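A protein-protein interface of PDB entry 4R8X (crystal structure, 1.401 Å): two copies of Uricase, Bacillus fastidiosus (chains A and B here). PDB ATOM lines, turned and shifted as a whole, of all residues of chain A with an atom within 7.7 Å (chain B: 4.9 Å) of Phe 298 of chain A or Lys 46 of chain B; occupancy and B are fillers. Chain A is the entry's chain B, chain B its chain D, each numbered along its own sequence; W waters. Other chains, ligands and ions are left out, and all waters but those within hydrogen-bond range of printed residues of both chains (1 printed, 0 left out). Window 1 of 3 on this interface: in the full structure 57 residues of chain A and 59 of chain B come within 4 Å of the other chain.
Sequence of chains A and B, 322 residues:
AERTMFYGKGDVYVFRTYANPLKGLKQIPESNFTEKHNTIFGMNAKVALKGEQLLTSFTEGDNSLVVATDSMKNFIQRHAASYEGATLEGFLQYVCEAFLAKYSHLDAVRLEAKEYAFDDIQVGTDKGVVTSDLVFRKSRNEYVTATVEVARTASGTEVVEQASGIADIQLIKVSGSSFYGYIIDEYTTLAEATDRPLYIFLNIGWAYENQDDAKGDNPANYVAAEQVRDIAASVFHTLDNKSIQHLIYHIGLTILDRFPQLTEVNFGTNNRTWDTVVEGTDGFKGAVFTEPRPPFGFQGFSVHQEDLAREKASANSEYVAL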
ATOM      1  N   PHE A 201     -18.341 -11.307   7.304  1.00  0.00           N
ATOM      2  CA  PHE A 201     -18.631 -11.304   5.878  1.00  0.00           C
ATOM      3  C   PHE A 201     -18.047 -12.605   5.341  1.00  0.00           C
ATOM      4  O   PHE A 201     -16.936 -12.987   5.733  1.00  0.00           O
ATOM      5  CB  PHE A 201     -17.960 -10.128   5.164  1.00  0.00           C
ATOM      6  CG  PHE A 201     -18.503  -8.761   5.524  1.00  0.00           C
ATOM      7  CD1 PHE A 201     -19.522  -8.583   6.450  1.00  0.00           C
ATOM      8  CD2 PHE A 201     -17.985  -7.637   4.887  1.00  0.00           C
ATOM      9  CE1 PHE A 201     -19.996  -7.296   6.746  1.00  0.00           C
ATOM     10  CE2 PHE A 201     -18.445  -6.372   5.181  1.00  0.00           C
ATOM     11  CZ  PHE A 201     -19.455  -6.198   6.103  1.00  0.00           C
ATOM     12  N   ILE A 244     -13.712 -17.568  13.822  1.00  0.00           N
ATOM     13  CA  ILE A 244     -14.171 -17.618  12.439  1.00  0.00           C
ATOM     14  C   ILE A 244     -13.499 -18.779  11.706  1.00  0.00           C
ATOM     15  O   ILE A 244     -14.135 -19.450  10.889  1.00  0.00           O
ATOM     16  CB  ILE A 244     -13.915 -16.306  11.677  1.00  0.00           C
ATOM     17  CG1 ILE A 244     -14.676 -15.155  12.324  1.00  0.00           C
ATOM     18  CG2 ILE A 244     -14.357 -16.442  10.226  1.00  0.00           C
ATOM     19  CD1 ILE A 244     -14.424 -13.820  11.665  1.00  0.00           C
ATOM     20  N   GLN A 245     -12.219 -19.009  12.011  1.00  0.00           N
ATOM     21  CA  GLN A 245     -11.455 -20.095  11.411  1.00  0.00           C
ATOM     22  C   GLN A 245     -12.167 -21.427  11.643  1.00  0.00           C
ATOM     23  O   GLN A 245     -12.374 -22.213  10.720  1.00  0.00           O
ATOM     24  CB  GLN A 245     -10.052 -20.172  12.041  1.00  0.00           C
ATOM     25  CG  GLN A 245      -9.054 -19.080  11.612  1.00  0.00           C
ATOM     26  CD  GLN A 245      -9.068 -17.858  12.510  1.00  0.00           C
ATOM     27  OE1 GLN A 245     -10.119 -17.444  13.005  1.00  0.00           O
ATOM     28  NE2 GLN A 245      -7.895 -17.272  12.726  1.00  0.00           N
ATOM     29  N   ILE A 248     -15.674 -21.591   9.725  1.00  0.00           N
ATOM     30  CA  ILE A 248     -15.656 -21.876   8.293  1.00  0.00           C
ATOM     31  C   ILE A 248     -15.222 -23.316   8.011  1.00  0.00           C
ATOM     32  O   ILE A 248     -15.652 -23.915   7.023  1.00  0.00           O
ATOM     33  CB  ILE A 248     -14.839 -20.848   7.473  1.00  0.00           C
ATOM     34  CG1 ILE A 248     -13.366 -20.851   7.897  1.00  0.00           C
ATOM     35  CG2 ILE A 248     -15.459 -19.462   7.605  1.00  0.00           C
ATOM     36  CD1 ILE A 248     -12.508 -19.888   7.078  1.00  0.00           C
ATOM     37  N   GLY A 268     -13.372 -16.855   1.740  1.00  0.00           N
ATOM     38  CA  GLY A 268     -12.719 -15.607   2.073  1.00  0.00           C
ATOM     39  C   GLY A 268     -13.643 -14.890   3.034  1.00  0.00           C
ATOM     40  O   GLY A 268     -14.827 -14.726   2.738  1.00  0.00           O
ATOM     41  N   THR A 269     -13.123 -14.490   4.187  1.00  0.00           N
ATOM     42  CA  THR A 269     -13.945 -13.883   5.233  1.00  0.00           C
ATOM     43  C   THR A 269     -13.467 -12.496   5.616  1.00  0.00           C
ATOM     44  O   THR A 269     -12.330 -12.125   5.354  1.00  0.00           O
ATOM     45  CB  THR A 269     -13.828 -14.669   6.525  1.00  0.00           C
ATOM     46  OG1 THR A 269     -12.541 -14.391   7.098  1.00  0.00           O
ATOM     47  CG2 THR A 269     -13.916 -16.155   6.264  1.00  0.00           C
ATOM     48  N   ASN A 270     -14.350 -11.742   6.266  1.00  0.00           N
ATOM     49  CA  ASN A 270     -13.947 -10.586   7.068  1.00  0.00           C
ATOM     50  C   ASN A 270     -14.544 -10.736   8.455  1.00  0.00           C
ATOM     51  O   ASN A 270     -15.701 -11.170   8.591  1.00  0.00           O
ATOM     52  CB  ASN A 270     -14.522  -9.263   6.553  1.00  0.00           C
ATOM     53  CG  ASN A 270     -13.956  -8.818   5.235  1.00  0.00           C
ATOM     54  OD1 ASN A 270     -14.410  -7.809   4.692  1.00  0.00           O
ATOM     55  ND2 ASN A 270     -12.978  -9.541   4.709  1.00  0.00           N
ATOM     56  N   ASN A 271     -13.796 -10.317   9.475  1.00  0.00           N
ATOM     57  CA  ASN A 271     -14.371 -10.072  10.794  1.00  0.00           C
ATOM     58  C   ASN A 271     -14.726  -8.582  10.882  1.00  0.00           C
ATOM     59  O   ASN A 271     -13.845  -7.732  10.788  1.00  0.00           O
ATOM     60  CB  ASN A 271     -13.390 -10.460  11.905  1.00  0.00           C
ATOM     61  CG  ASN A 271     -14.022 -10.428  13.276  1.00  0.00           C
ATOM     62  OD1 ASN A 271     -14.980  -9.697  13.507  1.00  0.00           O
ATOM     63  ND2 ASN A 271     -13.499 -11.224  14.193  1.00  0.00           N
ATOM     64  N   PRO A 295      -9.517  -1.357  10.433  1.00  0.00           N
ATOM     65  CA  PRO A 295      -8.855  -2.641  10.183  1.00  0.00           C
ATOM     66  C   PRO A 295      -9.762  -3.841  10.457  1.00  0.00           C
ATOM     67  O   PRO A 295     -10.499  -3.876  11.452  1.00  0.00           O
ATOM     68  CB  PRO A 295      -7.670  -2.604  11.154  1.00  0.00           C
ATOM     69  CG  PRO A 295      -7.362  -1.167  11.276  1.00  0.00           C
ATOM     70  CD  PRO A 295      -8.710  -0.510  11.325  1.00  0.00           C
ATOM     71  N   PHE A 296      -9.719  -4.813   9.548  1.00  0.00           N
ATOM     72  CA  PHE A 296     -10.572  -5.979   9.646  1.00  0.00           C
ATOM     73  C   PHE A 296      -9.757  -7.274   9.566  1.00  0.00           C
ATOM     74  O   PHE A 296      -8.858  -7.417   8.724  1.00  0.00           O
ATOM     75  CB  PHE A 296     -11.668  -5.969   8.564  1.00  0.00           C
ATOM     76  CG  PHE A 296     -11.144  -6.046   7.149  1.00  0.00           C
ATOM     77  CD1 PHE A 296     -10.950  -7.274   6.524  1.00  0.00           C
ATOM     78  CD2 PHE A 296     -10.841  -4.892   6.448  1.00  0.00           C
ATOM     79  CE1 PHE A 296     -10.484  -7.350   5.208  1.00  0.00           C
ATOM     80  CE2 PHE A 296     -10.355  -4.957   5.139  1.00  0.00           C
ATOM     81  CZ  PHE A 296     -10.175  -6.194   4.522  1.00  0.00           C
ATOM     82  N   GLY A 297     -10.079  -8.214  10.437  1.00  0.00           N
ATOM     83  CA  GLY A 297      -9.470  -9.528  10.351  1.00  0.00           C
ATOM     84  C   GLY A 297     -10.010 -10.224   9.122  1.00  0.00           C
ATOM     85  O   GLY A 297     -11.144  -9.966   8.700  1.00  0.00           O
ATOM     86  N   PHE A 298      -9.199 -11.095   8.532  1.00  0.00           N
ATOM     87  CA  PHE A 298      -9.660 -11.900   7.409  1.00  0.00           C
ATOM     88  C   PHE A 298      -9.014 -13.266   7.392  1.00  0.00           C
ATOM     89  O   PHE A 298      -7.936 -13.476   7.962  1.00  0.00           O
ATOM     90  CB  PHE A 298      -9.465 -11.191   6.066  1.00  0.00           C
ATOM     91  CG  PHE A 298      -8.035 -11.051   5.636  1.00  0.00           C
ATOM     92  CD1 PHE A 298      -7.426 -12.017   4.843  1.00  0.00           C
ATOM     93  CD2 PHE A 298      -7.303  -9.934   6.001  1.00  0.00           C
ATOM     94  CE1 PHE A 298      -6.105 -11.874   4.445  1.00  0.00           C
ATOM     95  CE2 PHE A 298      -5.988  -9.777   5.598  1.00  0.00           C
ATOM     96  CZ  PHE A 298      -5.390 -10.745   4.818  1.00  0.00           C
ATOM     97  N   GLN A 299      -9.713 -14.201   6.763  1.00  0.00           N
ATOM     98  CA  GLN A 299      -9.221 -15.562   6.625  1.00  0.00           C
ATOM     99  C   GLN A 299      -9.458 -16.052   5.212  1.00  0.00           C
ATOM    100  O   GLN A 299     -10.423 -15.646   4.561  1.00  0.00           O
ATOM    101  CB  GLN A 299      -9.933 -16.500   7.602  1.00  0.00           C
ATOM    102  CG  GLN A 299      -9.666 -16.234   9.074  1.00  0.00           C
ATOM    103  CD  GLN A 299     -10.493 -15.102   9.659  1.00  0.00           C
ATOM    104  OE1 GLN A 299     -11.574 -14.772   9.162  1.00  0.00           O
ATOM    105  NE2 GLN A 299      -9.981 -14.501  10.728  1.00  0.00           N
ATOM    106  N   GLY A 300      -8.564 -16.918   4.748  1.00  0.00           N
ATOM    107  CA  GLY A 300      -8.706 -17.627   3.487  1.00  0.00           C
ATOM    108  C   GLY A 300      -8.445 -19.097   3.770  1.00  0.00           C
ATOM    109  O   GLY A 300      -7.453 -19.435   4.406  1.00  0.00           O
ATOM    110  N   PHE B   6      -4.604 -19.050   4.981  1.00  0.00           N
ATOM    111  CA  PHE B   6      -3.939 -17.840   5.453  1.00  0.00           C
ATOM    112  C   PHE B   6      -4.912 -17.034   6.306  1.00  0.00           C
ATOM    113  O   PHE B   6      -6.117 -17.271   6.276  1.00  0.00           O
ATOM    114  CB  PHE B   6      -3.402 -16.987   4.295  1.00  0.00           C
ATOM    115  CG  PHE B   6      -4.449 -16.588   3.286  1.00  0.00           C
ATOM    116  CD1 PHE B   6      -5.271 -15.492   3.505  1.00  0.00           C
ATOM    117  CD2 PHE B   6      -4.603 -17.301   2.111  1.00  0.00           C
ATOM    118  CE1 PHE B   6      -6.240 -15.116   2.572  1.00  0.00           C
ATOM    119  CE2 PHE B   6      -5.559 -16.930   1.182  1.00  0.00           C
ATOM    120  CZ  PHE B   6      -6.376 -15.836   1.410  1.00  0.00           C
ATOM    121  N   TYR B   7      -4.393 -16.092   7.079  1.00  0.00           N
ATOM    122  CA  TYR B   7      -5.270 -15.177   7.793  1.00  0.00           C
ATOM    123  C   TYR B   7      -4.485 -13.902   8.084  1.00  0.00           C
ATOM    124  O   TYR B   7      -3.250 -13.901   8.052  1.00  0.00           O
ATOM    125  CB  TYR B   7      -5.826 -15.819   9.071  1.00  0.00           C
ATOM    126  CG  TYR B   7      -4.893 -15.747  10.245  1.00  0.00           C
ATOM    127  CD1 TYR B   7      -3.684 -16.436  10.245  1.00  0.00           C
ATOM    128  CD2 TYR B   7      -5.223 -14.992  11.360  1.00  0.00           C
ATOM    129  CE1 TYR B   7      -2.830 -16.370  11.322  1.00  0.00           C
ATOM    130  CE2 TYR B   7      -4.388 -14.927  12.437  1.00  0.00           C
ATOM    131  CZ  TYR B   7      -3.184 -15.606  12.408  1.00  0.00           C
ATOM    132  OH  TYR B   7      -2.334 -15.526  13.477  1.00  0.00           O
ATOM    133  N   GLY B   8      -5.190 -12.812   8.364  1.00  0.00           N
ATOM    134  CA  GLY B   8      -4.495 -11.571   8.605  1.00  0.00           C
ATOM    135  C   GLY B   8      -5.384 -10.393   8.924  1.00  0.00           C
ATOM    136  O   GLY B   8      -6.502 -10.565   9.415  1.00  0.00           O
ATOM    137  N   LYS B   9      -4.864  -9.198   8.652  1.00  0.00           N
ATOM    138  CA  LYS B   9      -5.585  -7.952   8.892  1.00  0.00           C
ATOM    139  C   LYS B   9      -5.518  -7.113   7.639  1.00  0.00           C
ATOM    140  O   LYS B   9      -4.443  -6.895   7.091  1.00  0.00           O
ATOM    141  CB  LYS B   9      -4.949  -7.192  10.057  1.00  0.00           C
ATOM    142  CG  LYS B   9      -5.833  -6.116  10.665  1.00  0.00           C
ATOM    143  CD  LYS B   9      -6.950  -6.725  11.484  1.00  0.00           C
ATOM    144  CE  LYS B   9      -7.240  -5.933  12.729  1.00  0.00           C
ATOM    145  NZ  LYS B   9      -8.257  -6.652  13.537  1.00  0.00           N
ATOM    146  N   GLY B  10      -6.674  -6.620   7.209  1.00  0.00           N
ATOM    147  CA  GLY B  10      -6.752  -5.707   6.079  1.00  0.00           C
ATOM    148  C   GLY B  10      -7.140  -4.315   6.526  1.00  0.00           C
ATOM    149  O   GLY B  10      -7.528  -4.135   7.678  1.00  0.00           O
ATOM    150  N   ASN B  44      -2.556   2.061   2.954  1.00  0.00           N
ATOM    151  CA  ASN B  44      -3.491   1.076   3.431  1.00  0.00           C
ATOM    152  C   ASN B  44      -2.799  -0.271   3.228  1.00  0.00           C
ATOM    153  O   ASN B  44      -2.655  -0.721   2.090  1.00  0.00           O
ATOM    154  CB  ASN B  44      -4.781   1.157   2.606  1.00  0.00           C
ATOM    155  CG  ASN B  44      -5.810   0.130   3.021  1.00  0.00           C
ATOM    156  OD1 ASN B  44      -5.483  -0.872   3.653  1.00  0.00           O
ATOM    157  ND2 ASN B  44      -7.073   0.370   2.660  1.00  0.00           N
ATOM    158  N   ALA B  45      -2.382  -0.897   4.329  1.00  0.00           N
ATOM    159  CA  ALA B  45      -1.666  -2.166   4.276  1.00  0.00           C
ATOM    160  C   ALA B  45      -2.561  -3.361   4.592  1.00  0.00           C
ATOM    161  O   ALA B  45      -3.526  -3.254   5.352  1.00  0.00           O
ATOM    162  CB  ALA B  45      -0.462  -2.145   5.218  1.00  0.00           C
ATOM    163  N   LYS B  46      -2.214  -4.507   4.014  1.00  0.00           N
ATOM    164  CA  LYS B  46      -2.933  -5.754   4.226  1.00  0.00           C
ATOM    165  C   LYS B  46      -1.903  -6.846   4.433  1.00  0.00           C
ATOM    166  O   LYS B  46      -1.051  -7.082   3.567  1.00  0.00           O
ATOM    167  CB  LYS B  46      -3.804  -6.077   3.011  1.00  0.00           C
ATOM    168  CG  LYS B  46      -4.678  -7.307   3.177  1.00  0.00           C
ATOM    169  CD  LYS B  46      -5.516  -7.548   1.928  1.00  0.00           C
ATOM    170  CE  LYS B  46      -6.460  -8.724   2.110  1.00  0.00           C
ATOM    171  NZ  LYS B  46      -7.584  -8.639   1.130  1.00  0.00           N
ATOM    172  N   VAL B  47      -1.973  -7.500   5.586  1.00  0.00           N
ATOM    173  CA  VAL B  47      -1.002  -8.539   5.927  1.00  0.00           C
ATOM    174  C   VAL B  47      -1.668  -9.896   6.008  1.00  0.00           C
ATOM    175  O   VAL B  47      -2.760 -10.021   6.558  1.00  0.00           O
ATOM    176  CB  VAL B  47      -0.270  -8.240   7.266  1.00  0.00           C
ATOM    177  CG1 VAL B  47      -1.253  -8.038   8.424  1.00  0.00           C
ATOM    178  CG2 VAL B  47       0.745  -9.340   7.587  1.00  0.00           C
ATOM    179  N   ALA B  48      -1.013 -10.906   5.434  1.00  0.00           N
ATOM    180  CA  ALA B  48      -1.468 -12.284   5.530  1.00  0.00           C
ATOM    181  C   ALA B  48      -0.335 -13.134   6.082  1.00  0.00           C
ATOM    182  O   ALA B  48       0.803 -13.035   5.605  1.00  0.00           O
ATOM    183  CB  ALA B  48      -1.894 -12.804   4.162  1.00  0.00           C
ATOM    184  N   THR B  69      -5.117 -10.770  15.106  1.00  0.00           N
ATOM    185  CA  THR B  69      -5.071  -9.825  13.984  1.00  0.00           C
ATOM    186  C   THR B  69      -4.815  -8.393  14.469  1.00  0.00           C
ATOM    187  O   THR B  69      -4.084  -7.626  13.829  1.00  0.00           O
ATOM    188  CB  THR B  69      -6.324  -9.906  13.050  1.00  0.00           C
ATOM    189  OG1 THR B  69      -7.491  -9.459  13.748  1.00  0.00           O
ATOM    190  CG2 THR B  69      -6.527 -11.331  12.526  1.00  0.00           C
ATOM    191  N   ARG B 110       2.873 -12.198   3.779  1.00  0.00           N
ATOM    192  CA  ARG B 110       2.591 -11.390   2.599  1.00  0.00           C
ATOM    193  C   ARG B 110       2.052 -10.032   3.000  1.00  0.00           C
ATOM    194  O   ARG B 110       1.085  -9.945   3.756  1.00  0.00           O
ATOM    195  CB  ARG B 110       1.530 -12.086   1.742  1.00  0.00           C
ATOM    196  CG  ARG B 110       1.149 -11.340   0.468  1.00  0.00           C
ATOM    197  CD  ARG B 110       0.063 -12.096  -0.282  1.00  0.00           C
ATOM    198  NE  ARG B 110      -0.284 -11.491  -1.569  1.00  0.00           N
ATOM    199  CZ  ARG B 110       0.378 -11.732  -2.691  1.00  0.00           C
ATOM    200  NH1 ARG B 110       1.420 -12.553  -2.670  1.00  0.00           N
ATOM    201  NH2 ARG B 110       0.010 -11.162  -3.833  1.00  0.00           N
ATOM    202  N   LEU B 111       2.677  -8.983   2.490  1.00  0.00           N
ATOM    203  CA  LEU B 111       2.172  -7.625   2.669  1.00  0.00           C
ATOM    204  C   LEU B 111       1.793  -7.032   1.328  1.00  0.00           C
ATOM    205  O   LEU B 111       2.553  -7.127   0.362  1.00  0.00           O
ATOM    206  CB  LEU B 111       3.230  -6.733   3.319  1.00  0.00           C
ATOM    207  CG  LEU B 111       3.213  -6.515   4.827  1.00  0.00           C
ATOM    208  CD1 LEU B 111       1.973  -5.727   5.258  1.00  0.00           C
ATOM    209  CD2 LEU B 111       3.357  -7.852   5.567  1.00  0.00           C
ATOM    210  N   GLU B 112       0.608  -6.429   1.284  1.00  0.00           N
ATOM    211  CA  GLU B 112       0.158  -5.652   0.135  1.00  0.00           C
ATOM    212  C   GLU B 112      -0.102  -4.230   0.612  1.00  0.00           C
ATOM    213  O   GLU B 112      -0.545  -4.026   1.744  1.00  0.00           O
ATOM    214  CB  GLU B 112      -1.138  -6.232  -0.423  1.00  0.00           C
ATOM    215  CG  GLU B 112      -0.987  -7.640  -0.951  1.00  0.00           C
ATOM    216  CD  GLU B 112      -2.304  -8.270  -1.360  1.00  0.00           C
ATOM    217  OE1 GLU B 112      -3.330  -7.555  -1.411  1.00  0.00           O
ATOM    218  OE2 GLU B 112      -2.313  -9.490  -1.623  1.00  0.00           O
HETATM  219  O   HOH W   1     -11.211  -7.245  12.914  1.00  0.00           O
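N of Gln 299 of chain A is in hydrogen-bond range of OG1 of Thr 269 of chain A, at 2.9 Å.
The backbone NH (N) of Asn 271 of chain A is in hydrogen-bond range of the backbone carbonyl oxygen (O) of Gly 297 of chain A (2.8 Å).
The backbone carbonyl oxygen of Lys 9 of chain B lies within hydrogen-bond range of the backbone NH of Val 47 of chain B (3.0 Å).
The side-chain hydroxyl (OG1) of Thr 69 of chain B sits at hydrogen-bond distance from the side-chain amino group (NZ) of Lys 9 of chain B (2.9 Å).
N of Lys 46 of chain B lies within hydrogen-bond range of O of Glu 112 of chain B.
Of the 14 printed residues of chain B, 8 touch a printed residue of chain A.
Hydrophobic or aromatic side chains of chain B within 4 Å of the printed part of chain A: Phe 6 and Tyr 7.
Of the 14 printed residues of chain A, 7 touch a printed residue of chain B.
Printed residues of chain A that touch a printed residue of chain B: Gln 245, Pro 295, Phe 296, Gly 297, Phe 298, Gln 299 and Gly 300.
Among the printed residues, 19 pairs touch across the chains.
The backbone NH (N) of Gly 10 of chain B is in hydrogen-bond range of the backbone carbonyl oxygen (O) of Phe 296 of chain A, at 2.8 Å.
O of Phe 298 of chain A sits at hydrogen-bond distance from N of Gly 8 of chain B, at 2.9 Å.
N of Gly 300 of chain A sits at hydrogen-bond distance from O of Phe 6 of chain B.
Water W1 lies within hydrogen-bond range of N of Gly 297 of chain A (2.9 Å), NZ of Lys 9 of chain B (3.1 Å) and O of Asn 271 of chain A (3.4 Å).
CD2 of Tyr 7 of chain B touches NE2 of Gln 245 of chain A, at 3.8 Å.
O of Gly 8 of chain B touches O of Phe 296 of chain A, 3.99 Å away.
Gly 297 of chain A touches Gly 8 of chain B (CA to O, 3.3 Å).
CE1 of Phe 298 of chain A touches CE1 of Phe 6 of chain B (3.7 Å).
Phe 298 of chain A touches Tyr 7 of chain B.
Phe 298 of chain A touches Lys 9 of chain B (CE2 to N, 3.3 Å).
Gly 10 of chain B touches Phe 298 of chain A.
CE of Lys 46 of chain B touches CZ of Phe 298 of chain A (3.5 Å).
Phe 6 of chain B touches Gln 299 of chain A.
CB of Tyr 7 of chain B touches CG of Gln 299 of chain A (3.9 Å).
Of the printed residues of chain B, Phe 298 of chain A touches Phe 6 (3.7 Å), Tyr 7 (3.2 Å), Gly 8 (2.9 Å), Lys 9 (3.3 Å), Gly 10 (3.6 Å), Lys 46 (3.5 Å) and Val 47 (3.2 Å).
No residue of chain A comes within 4 Å of Ala 45 of chain B.
Printed residues of chain B within 4 Å of Phe 296 of chain A: Gly 8, Lys 9 and Gly 10.
Of the printed residues of chain B, Pro 295 of chain A touches Lys 9 (3.7 Å) and Gly 10 (3.2 Å).
The nearest residue of chain B that does not touch Phe 298 of chain A is Ala 48 of chain B (4.1 Å).
The nearest residue of chain A that does not touch Lys 46 of chain B is Phe 296 of chain A (4.9 Å).
No position is printed for both chains.
Of the 19 pairs that touch across the chains among the printed residues, none has its exchanged pair printed and touching as well.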
